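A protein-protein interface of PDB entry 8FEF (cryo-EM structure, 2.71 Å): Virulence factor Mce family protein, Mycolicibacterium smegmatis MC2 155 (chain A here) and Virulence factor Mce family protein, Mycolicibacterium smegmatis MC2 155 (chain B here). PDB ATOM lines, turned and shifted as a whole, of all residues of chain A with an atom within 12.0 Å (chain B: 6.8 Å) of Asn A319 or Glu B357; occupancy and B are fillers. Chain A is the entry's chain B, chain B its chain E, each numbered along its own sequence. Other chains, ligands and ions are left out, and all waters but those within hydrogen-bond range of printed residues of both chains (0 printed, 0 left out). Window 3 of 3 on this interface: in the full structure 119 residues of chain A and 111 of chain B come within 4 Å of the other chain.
Among the printed residues, pairs that only touch across the chains: Val A327 with Arg B362 (3.4 Å), Asn A319 with Thr B335 (3.7 Å), Asn A319 with Leu B336 (3.8 Å), Asn A319 with Glu B357 (3.9 Å) and Lys A317 with Thr B335 (3.96 Å).
The backbone carbonyl oxygen of Thr B335 lies within hydrogen-bond range of the side-chain hydroxyl of Ser B338 (2.7 Å).
The backbone NH (N) of Ser B337 lies within hydrogen-bond range of the side-chain carboxylate (OE1) of Glu B357 (2.8 Å).
OG of Ser B337 lies within hydrogen-bond range of NH2 of Arg B362 (3.4 Å).
OE2 of Glu B357 lies within salt-bridge range of NH2 of Arg B362 (3.1 Å).
Asn A319 touches three residues of chain B.
Glu B357 touches one residue of chain A.
Of chain A, only Lys A317 (3.96 Å) and Asn A319 (3.7 Å) come within 4 Å of Thr B335.
Of chain A, only Asn A319 comes within 4 Å of Leu B336.
No residue of chain A comes within 4 Å of Leu B353.
No residue of chain A comes within 4 Å of Arg B354.
No residue of chain A comes within 4 Å of Leu B356.
No residue of chain A comes within 4 Å of Gln B358.
No residue of chain A comes within 4 Å of Trp B360.
No residue of chain A comes within 4 Å of Gly B361.
Of the printed residues of chain B, Lys A317 touches Leu B334 and Thr B335.
Printed residues of chain A within 4 Å of Leu B334: Lys A317.
Of the printed residues of chain B, Val A327 touches Arg B362.
The nearest residue of chain B that does not touch Asn A319 is Leu B334 (4.3 Å).
The nearest residue of chain A that does not touch Glu B357 is Val A327 (5.7 Å).
The nearest printed residue of chain B that does not touch Val A327 is Thr B335 (5.1 Å).
Printed residues of chain B that touch a printed residue of chain A: Leu B334, Thr B335, Leu B336, Glu B357 and Arg B362.
Hydrophobic or aromatic side chains of chain B that line the printed part of chain A: Leu B334.
Of the 10 printed residues of chain A, 3 touch a printed residue of chain B.
Hydrophobic or aromatic side chains of chain A within 4 Å of the printed part of chain B: Val A327.
Among the printed residues, no Asp or Glu carboxylate lies within 4 Å of a Lys or Arg side-chain nitrogen of the other chain.
O of Lys A317 sits at hydrogen-bond distance from N of Leu B334, 2.8 Å away.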
ATOM      1  N   THR A 315      21.529  17.719   0.120  1.00  0.00           N
ATOM      2  CA  THR A 315      20.155  17.894  -0.319  1.00  0.00           C
ATOM      3  C   THR A 315      19.873  19.376  -0.512  1.00  0.00           C
ATOM      4  O   THR A 315      20.324  20.207   0.279  1.00  0.00           O
ATOM      5  CB  THR A 315      19.167  17.349   0.720  1.00  0.00           C
ATOM      6  OG1 THR A 315      19.365  18.042   1.954  1.00  0.00           O
ATOM      7  CG2 THR A 315      19.414  15.881   0.982  1.00  0.00           C
ATOM      8  N   LEU A 316      19.121  19.698  -1.559  1.00  0.00           N
ATOM      9  CA  LEU A 316      18.848  21.078  -1.935  1.00  0.00           C
ATOM     10  C   LEU A 316      17.477  21.496  -1.423  1.00  0.00           C
ATOM     11  O   LEU A 316      16.502  20.752  -1.549  1.00  0.00           O
ATOM     12  CB  LEU A 316      18.921  21.261  -3.452  1.00  0.00           C
ATOM     13  CG  LEU A 316      20.256  21.720  -4.047  1.00  0.00           C
ATOM     14  CD1 LEU A 316      21.428  20.905  -3.522  1.00  0.00           C
ATOM     15  CD2 LEU A 316      20.204  21.657  -5.565  1.00  0.00           C
ATOM     16  N   LYS A 317      17.410  22.689  -0.842  1.00  0.00           N
ATOM     17  CA  LYS A 317      16.159  23.272  -0.378  1.00  0.00           C
ATOM     18  C   LYS A 317      15.827  24.464  -1.266  1.00  0.00           C
ATOM     19  O   LYS A 317      16.632  25.395  -1.383  1.00  0.00           O
ATOM     20  CB  LYS A 317      16.260  23.693   1.088  1.00  0.00           C
ATOM     21  CG  LYS A 317      15.000  24.336   1.638  1.00  0.00           C
ATOM     22  CD  LYS A 317      15.192  24.763   3.079  1.00  0.00           C
ATOM     23  CE  LYS A 317      13.929  25.388   3.641  1.00  0.00           C
ATOM     24  NZ  LYS A 317      14.097  25.789   5.063  1.00  0.00           N
ATOM     25  N   LEU A 318      14.652  24.434  -1.888  1.00  0.00           N
ATOM     26  CA  LEU A 318      14.255  25.496  -2.802  1.00  0.00           C
ATOM     27  C   LEU A 318      12.742  25.493  -2.944  1.00  0.00           C
ATOM     28  O   LEU A 318      12.072  24.504  -2.639  1.00  0.00           O
ATOM     29  CB  LEU A 318      14.937  25.341  -4.167  1.00  0.00           C
ATOM     30  CG  LEU A 318      14.903  23.979  -4.872  1.00  0.00           C
ATOM     31  CD1 LEU A 318      13.674  23.825  -5.753  1.00  0.00           C
ATOM     32  CD2 LEU A 318      16.169  23.776  -5.685  1.00  0.00           C
ATOM     33  N   ASN A 319      12.215  26.618  -3.416  1.00  0.00           N
ATOM     34  CA  ASN A 319      10.780  26.761  -3.637  1.00  0.00           C
ATOM     35  C   ASN A 319      10.474  27.039  -5.104  1.00  0.00           C
ATOM     36  O   ASN A 319      11.228  26.634  -5.989  1.00  0.00           O
ATOM     37  CB  ASN A 319      10.209  27.877  -2.756  1.00  0.00           C
ATOM     38  CG  ASN A 319      11.032  29.147  -2.816  1.00  0.00           C
ATOM     39  OD1 ASN A 319      11.951  29.269  -3.624  1.00  0.00           O
ATOM     40  ND2 ASN A 319      10.704  30.102  -1.955  1.00  0.00           N
ATOM     41  N   VAL A 327       8.778  25.394  -1.050  1.00  0.00           N
ATOM     42  CA  VAL A 327       9.614  25.176   0.121  1.00  0.00           C
ATOM     43  C   VAL A 327       9.956  23.684   0.187  1.00  0.00           C
ATOM     44  O   VAL A 327      10.330  23.144   1.230  1.00  0.00           O
ATOM     45  CB  VAL A 327       8.909  25.697   1.405  1.00  0.00           C
ATOM     46  CG1 VAL A 327       7.731  24.805   1.802  1.00  0.00           C
ATOM     47  CG2 VAL A 327       9.901  25.893   2.553  1.00  0.00           C
ATOM     48  N   ARG A 328       9.848  23.027  -0.964  1.00  0.00           N
ATOM     49  CA  ARG A 328      10.140  21.605  -1.054  1.00  0.00           C
ATOM     50  C   ARG A 328      11.614  21.333  -0.777  1.00  0.00           C
ATOM     51  O   ARG A 328      12.479  22.188  -0.986  1.00  0.00           O
ATOM     52  CB  ARG A 328       9.762  21.067  -2.436  1.00  0.00           C
ATOM     53  CG  ARG A 328      10.670  21.538  -3.560  1.00  0.00           C
ATOM     54  CD  ARG A 328      10.328  20.845  -4.866  1.00  0.00           C
ATOM     55  NE  ARG A 328      11.338  21.078  -5.890  1.00  0.00           N
ATOM     56  CZ  ARG A 328      11.298  20.562  -7.110  1.00  0.00           C
ATOM     57  NH1 ARG A 328      10.303  19.781  -7.498  1.00  0.00           N
ATOM     58  NH2 ARG A 328      12.281  20.834  -7.963  1.00  0.00           N
ATOM     59  N   THR A 329      11.894  20.131  -0.284  1.00  0.00           N
ATOM     60  CA  THR A 329      13.256  19.680  -0.030  1.00  0.00           C
ATOM     61  C   THR A 329      13.592  18.585  -1.033  1.00  0.00           C
ATOM     62  O   THR A 329      12.897  17.566  -1.102  1.00  0.00           O
ATOM     63  CB  THR A 329      13.412  19.168   1.401  1.00  0.00           C
ATOM     64  OG1 THR A 329      12.479  18.107   1.637  1.00  0.00           O
ATOM     65  CG2 THR A 329      13.162  20.289   2.398  1.00  0.00           C
ATOM     66  N   VAL A 330      14.655  18.798  -1.801  1.00  0.00           N
ATOM     67  CA  VAL A 330      15.087  17.878  -2.846  1.00  0.00           C
ATOM     68  C   VAL A 330      16.369  17.200  -2.387  1.00  0.00           C
ATOM     69  O   VAL A 330      17.331  17.877  -2.003  1.00  0.00           O
ATOM     70  CB  VAL A 330      15.298  18.607  -4.184  1.00  0.00           C
ATOM     71  CG1 VAL A 330      15.663  17.616  -5.277  1.00  0.00           C
ATOM     72  CG2 VAL A 330      14.053  19.391  -4.557  1.00  0.00           C
ATOM     73  N   ARG A 331      16.383  15.871  -2.424  1.00  0.00           N
ATOM     74  CA  ARG A 331      17.520  15.091  -1.961  1.00  0.00           C
ATOM     75  C   ARG A 331      18.357  14.642  -3.150  1.00  0.00           C
ATOM     76  O   ARG A 331      17.839  14.012  -4.077  1.00  0.00           O
ATOM     77  CB  ARG A 331      17.034  13.879  -1.159  1.00  0.00           C
ATOM     78  CG  ARG A 331      18.122  12.985  -0.577  1.00  0.00           C
ATOM     79  CD  ARG A 331      18.348  11.727  -1.408  1.00  0.00           C
ATOM     80  NE  ARG A 331      17.149  10.903  -1.507  1.00  0.00           N
ATOM     81  CZ  ARG A 331      16.380  10.823  -2.584  1.00  0.00           C
ATOM     82  NH1 ARG A 331      16.661  11.498  -3.686  1.00  0.00           N
ATOM     83  NH2 ARG A 331      15.302  10.043  -2.555  1.00  0.00           N
ATOM     84  N   LEU B 334      18.239  27.708  -1.041  1.00  0.00           N
ATOM     85  CA  LEU B 334      18.036  28.615  -2.163  1.00  0.00           C
ATOM     86  C   LEU B 334      16.674  29.290  -2.081  1.00  0.00           C
ATOM     87  O   LEU B 334      16.174  29.806  -3.085  1.00  0.00           O
ATOM     88  CB  LEU B 334      18.192  27.874  -3.491  1.00  0.00           C
ATOM     89  CG  LEU B 334      19.520  27.138  -3.677  1.00  0.00           C
ATOM     90  CD1 LEU B 334      19.568  26.431  -5.022  1.00  0.00           C
ATOM     91  CD2 LEU B 334      20.687  28.099  -3.535  1.00  0.00           C
ATOM     92  N   THR B 335      16.066  29.281  -0.900  1.00  0.00           N
ATOM     93  CA  THR B 335      14.782  29.930  -0.688  1.00  0.00           C
ATOM     94  C   THR B 335      14.950  31.444  -0.817  1.00  0.00           C
ATOM     95  O   THR B 335      16.033  31.987  -0.590  1.00  0.00           O
ATOM     96  CB  THR B 335      14.247  29.529   0.693  1.00  0.00           C
ATOM     97  OG1 THR B 335      14.076  28.108   0.733  1.00  0.00           O
ATOM     98  CG2 THR B 335      12.906  30.148   0.985  1.00  0.00           C
ATOM     99  N   LEU B 336      13.861  32.127  -1.191  1.00  0.00           N
ATOM    100  CA  LEU B 336      13.925  33.568  -1.424  1.00  0.00           C
ATOM    101  C   LEU B 336      14.290  34.340  -0.161  1.00  0.00           C
ATOM    102  O   LEU B 336      14.929  35.393  -0.247  1.00  0.00           O
ATOM    103  CB  LEU B 336      12.596  34.069  -1.987  1.00  0.00           C
ATOM    104  CG  LEU B 336      12.198  33.546  -3.369  1.00  0.00           C
ATOM    105  CD1 LEU B 336      10.929  34.224  -3.853  1.00  0.00           C
ATOM    106  CD2 LEU B 336      13.324  33.734  -4.371  1.00  0.00           C
ATOM    107  N   SER B 337      13.899  33.840   1.012  1.00  0.00           N
ATOM    108  CA  SER B 337      14.276  34.501   2.259  1.00  0.00           C
ATOM    109  C   SER B 337      15.783  34.433   2.487  1.00  0.00           C
ATOM    110  O   SER B 337      16.414  35.430   2.863  1.00  0.00           O
ATOM    111  CB  SER B 337      13.523  33.870   3.429  1.00  0.00           C
ATOM    112  OG  SER B 337      13.834  32.493   3.550  1.00  0.00           O
ATOM    113  N   SER B 338      16.375  33.256   2.268  1.00  0.00           N
ATOM    114  CA  SER B 338      17.817  33.113   2.429  1.00  0.00           C
ATOM    115  C   SER B 338      18.570  33.914   1.376  1.00  0.00           C
ATOM    116  O   SER B 338      19.632  34.478   1.662  1.00  0.00           O
ATOM    117  CB  SER B 338      18.208  31.639   2.362  1.00  0.00           C
ATOM    118  OG  SER B 338      17.940  31.099   1.080  1.00  0.00           O
ATOM    119  N   MET B 352      12.609  43.069  -2.169  1.00  0.00           N
ATOM    120  CA  MET B 352      12.243  42.775  -3.550  1.00  0.00           C
ATOM    121  C   MET B 352      11.662  41.373  -3.681  1.00  0.00           C
ATOM    122  O   MET B 352      10.679  41.164  -4.402  1.00  0.00           O
ATOM    123  CB  MET B 352      13.456  42.942  -4.466  1.00  0.00           C
ATOM    124  CG  MET B 352      13.151  42.719  -5.940  1.00  0.00           C
ATOM    125  SD  MET B 352      14.559  43.037  -7.018  1.00  0.00           S
ATOM    126  CE  MET B 352      15.717  41.801  -6.441  1.00  0.00           C
ATOM    127  N   LEU B 353      12.255  40.398  -2.991  1.00  0.00           N
ATOM    128  CA  LEU B 353      11.808  39.016  -3.065  1.00  0.00           C
ATOM    129  C   LEU B 353      11.425  38.418  -1.720  1.00  0.00           C
ATOM    130  O   LEU B 353      10.715  37.407  -1.698  1.00  0.00           O
ATOM    131  CB  LEU B 353      12.882  38.133  -3.726  1.00  0.00           C
ATOM    132  CG  LEU B 353      14.159  37.676  -3.015  1.00  0.00           C
ATOM    133  CD1 LEU B 353      15.078  36.993  -4.016  1.00  0.00           C
ATOM    134  CD2 LEU B 353      14.895  38.802  -2.333  1.00  0.00           C
ATOM    135  N   ARG B 354      11.849  39.016  -0.605  1.00  0.00           N
ATOM    136  CA  ARG B 354      11.361  38.593   0.705  1.00  0.00           C
ATOM    137  C   ARG B 354       9.849  38.759   0.806  1.00  0.00           C
ATOM    138  O   ARG B 354       9.140  37.850   1.251  1.00  0.00           O
ATOM    139  CB  ARG B 354      12.059  39.396   1.801  1.00  0.00           C
ATOM    140  CG  ARG B 354      11.407  39.302   3.165  1.00  0.00           C
ATOM    141  CD  ARG B 354      11.854  38.060   3.902  1.00  0.00           C
ATOM    142  NE  ARG B 354      13.304  37.918   3.889  1.00  0.00           N
ATOM    143  CZ  ARG B 354      13.982  37.110   4.692  1.00  0.00           C
ATOM    144  NH1 ARG B 354      13.375  36.379   5.610  1.00  0.00           N
ATOM    145  NH2 ARG B 354      15.305  37.040   4.572  1.00  0.00           N
ATOM    146  N   ALA B 355       9.339  39.919   0.386  1.00  0.00           N
ATOM    147  CA  ALA B 355       7.897  40.136   0.377  1.00  0.00           C
ATOM    148  C   ALA B 355       7.215  39.335  -0.722  1.00  0.00           C
ATOM    149  O   ALA B 355       6.034  38.994  -0.595  1.00  0.00           O
ATOM    150  CB  ALA B 355       7.590  41.624   0.219  1.00  0.00           C
ATOM    151  N   LEU B 356       7.931  39.043  -1.810  1.00  0.00           N
ATOM    152  CA  LEU B 356       7.383  38.176  -2.849  1.00  0.00           C
ATOM    153  C   LEU B 356       7.125  36.774  -2.312  1.00  0.00           C
ATOM    154  O   LEU B 356       6.092  36.166  -2.609  1.00  0.00           O
ATOM    155  CB  LEU B 356       8.333  38.130  -4.045  1.00  0.00           C
ATOM    156  CG  LEU B 356       7.966  37.187  -5.191  1.00  0.00           C
ATOM    157  CD1 LEU B 356       6.670  37.624  -5.850  1.00  0.00           C
ATOM    158  CD2 LEU B 356       9.095  37.119  -6.208  1.00  0.00           C
ATOM    159  N   GLU B 357       8.058  36.248  -1.520  1.00  0.00           N
ATOM    160  CA  GLU B 357       7.872  34.930  -0.924  1.00  0.00           C
ATOM    161  C   GLU B 357       6.882  34.963   0.235  1.00  0.00           C
ATOM    162  O   GLU B 357       6.109  34.016   0.420  1.00  0.00           O
ATOM    163  CB  GLU B 357       9.210  34.375  -0.443  1.00  0.00           C
ATOM    164  CG  GLU B 357       9.109  32.965   0.092  1.00  0.00           C
ATOM    165  CD  GLU B 357      10.239  32.616   1.027  1.00  0.00           C
ATOM    166  OE1 GLU B 357      11.167  33.437   1.180  1.00  0.00           O
ATOM    167  OE2 GLU B 357      10.181  31.530   1.636  1.00  0.00           O
ATOM    168  N   GLN B 358       6.886  36.039   1.026  1.00  0.00           N
ATOM    169  CA  GLN B 358       5.970  36.121   2.159  1.00  0.00           C
ATOM    170  C   GLN B 358       4.525  36.283   1.703  1.00  0.00           C
ATOM    171  O   GLN B 358       3.607  35.797   2.375  1.00  0.00           O
ATOM    172  CB  GLN B 358       6.379  37.270   3.081  1.00  0.00           C
ATOM    173  CG  GLN B 358       5.563  37.374   4.360  1.00  0.00           C
ATOM    174  CD  GLN B 358       6.072  38.459   5.288  1.00  0.00           C
ATOM    175  OE1 GLN B 358       7.206  38.919   5.160  1.00  0.00           O
ATOM    176  NE2 GLN B 358       5.231  38.877   6.227  1.00  0.00           N
ATOM    177  N   ALA B 359       4.300  36.958   0.571  1.00  0.00           N
ATOM    178  CA  ALA B 359       2.954  37.054   0.019  1.00  0.00           C
ATOM    179  C   ALA B 359       2.416  35.699  -0.419  1.00  0.00           C
ATOM    180  O   ALA B 359       1.199  35.548  -0.576  1.00  0.00           O
ATOM    181  CB  ALA B 359       2.933  38.027  -1.160  1.00  0.00           C
ATOM    182  N   TRP B 360       3.291  34.715  -0.620  1.00  0.00           N
ATOM    183  CA  TRP B 360       2.878  33.351  -0.925  1.00  0.00           C
ATOM    184  C   TRP B 360       2.491  32.628   0.360  1.00  0.00           C
ATOM    185  O   TRP B 360       2.281  33.264   1.397  1.00  0.00           O
ATOM    186  CB  TRP B 360       3.989  32.599  -1.661  1.00  0.00           C
ATOM    187  CG  TRP B 360       4.391  33.228  -2.967  1.00  0.00           C
ATOM    188  CD1 TRP B 360       3.777  34.269  -3.600  1.00  0.00           C
ATOM    189  CD2 TRP B 360       5.498  32.853  -3.797  1.00  0.00           C
ATOM    190  NE1 TRP B 360       4.431  34.565  -4.770  1.00  0.00           N
ATOM    191  CE2 TRP B 360       5.491  33.711  -4.915  1.00  0.00           C
ATOM    192  CE3 TRP B 360       6.494  31.877  -3.703  1.00  0.00           C
ATOM    193  CZ2 TRP B 360       6.440  33.620  -5.930  1.00  0.00           C
ATOM    194  CZ3 TRP B 360       7.436  31.790  -4.713  1.00  0.00           C
ATOM    195  CH2 TRP B 360       7.402  32.656  -5.810  1.00  0.00           C
ATOM    196  N   GLY B 361       2.391  31.300   0.304  1.00  0.00           N
ATOM    197  CA  GLY B 361       1.951  30.537   1.460  1.00  0.00           C
ATOM    198  C   GLY B 361       2.936  30.492   2.613  1.00  0.00           C
ATOM    199  O   GLY B 361       2.554  30.051   3.702  1.00  0.00           O
ATOM    200  N   ARG B 362       4.179  30.922   2.402  1.00  0.00           N
ATOM    201  CA  ARG B 362       5.179  30.880   3.462  1.00  0.00           C
ATOM    202  C   ARG B 362       4.788  31.789   4.621  1.00  0.00           C
ATOM    203  O   ARG B 362       4.200  32.856   4.427  1.00  0.00           O
ATOM    204  CB  ARG B 362       6.550  31.280   2.915  1.00  0.00           C
ATOM    205  CG  ARG B 362       7.213  30.206   2.070  1.00  0.00           C
ATOM    206  CD  ARG B 362       8.106  29.319   2.927  1.00  0.00           C
ATOM    207  NE  ARG B 362       9.433  29.894   3.113  1.00  0.00           N
ATOM    208  CZ  ARG B 362      10.333  29.441   3.975  1.00  0.00           C
ATOM    209  NH1 ARG B 362      10.071  28.424   4.777  1.00  0.00           N
ATOM    210  NH2 ARG B 362      11.523  30.031   4.040  1.00  0.00           N
ATOM    211  N   ASP B 363       5.118  31.352   5.840  1.00  0.00           N
ATOM    212  CA  ASP B 363       4.801  32.064   7.065  1.00  0.00           C
ATOM    213  C   ASP B 363       6.073  32.612   7.701  1.00  0.00           C
ATOM    214  O   ASP B 363       7.116  31.951   7.652  1.00  0.00           O
ATOM    215  CB  ASP B 363       4.092  31.135   8.060  1.00  0.00           C
ATOM    216  CG  ASP B 363       3.557  31.869   9.273  1.00  0.00           C
ATOM    217  OD1 ASP B 363       2.563  32.610   9.129  1.00  0.00           O
ATOM    218  OD2 ASP B 363       4.131  31.707  10.370  1.00  0.00           O
ATOM    219  N   MET B 367      10.656  31.369   8.549  1.00  0.00           N
ATOM    220  CA  MET B 367      11.628  32.068   7.724  1.00  0.00           C
ATOM    221  C   MET B 367      12.757  32.616   8.585  1.00  0.00           C
ATOM    222  O   MET B 367      12.588  32.863   9.781  1.00  0.00           O
ATOM    223  CB  MET B 367      10.967  33.212   6.953  1.00  0.00           C
ATOM    224  CG  MET B 367       9.783  32.788   6.107  1.00  0.00           C
ATOM    225  SD  MET B 367       8.869  34.185   5.430  1.00  0.00           S
ATOM    226  CE  MET B 367      10.072  34.855   4.290  1.00  0.00           C
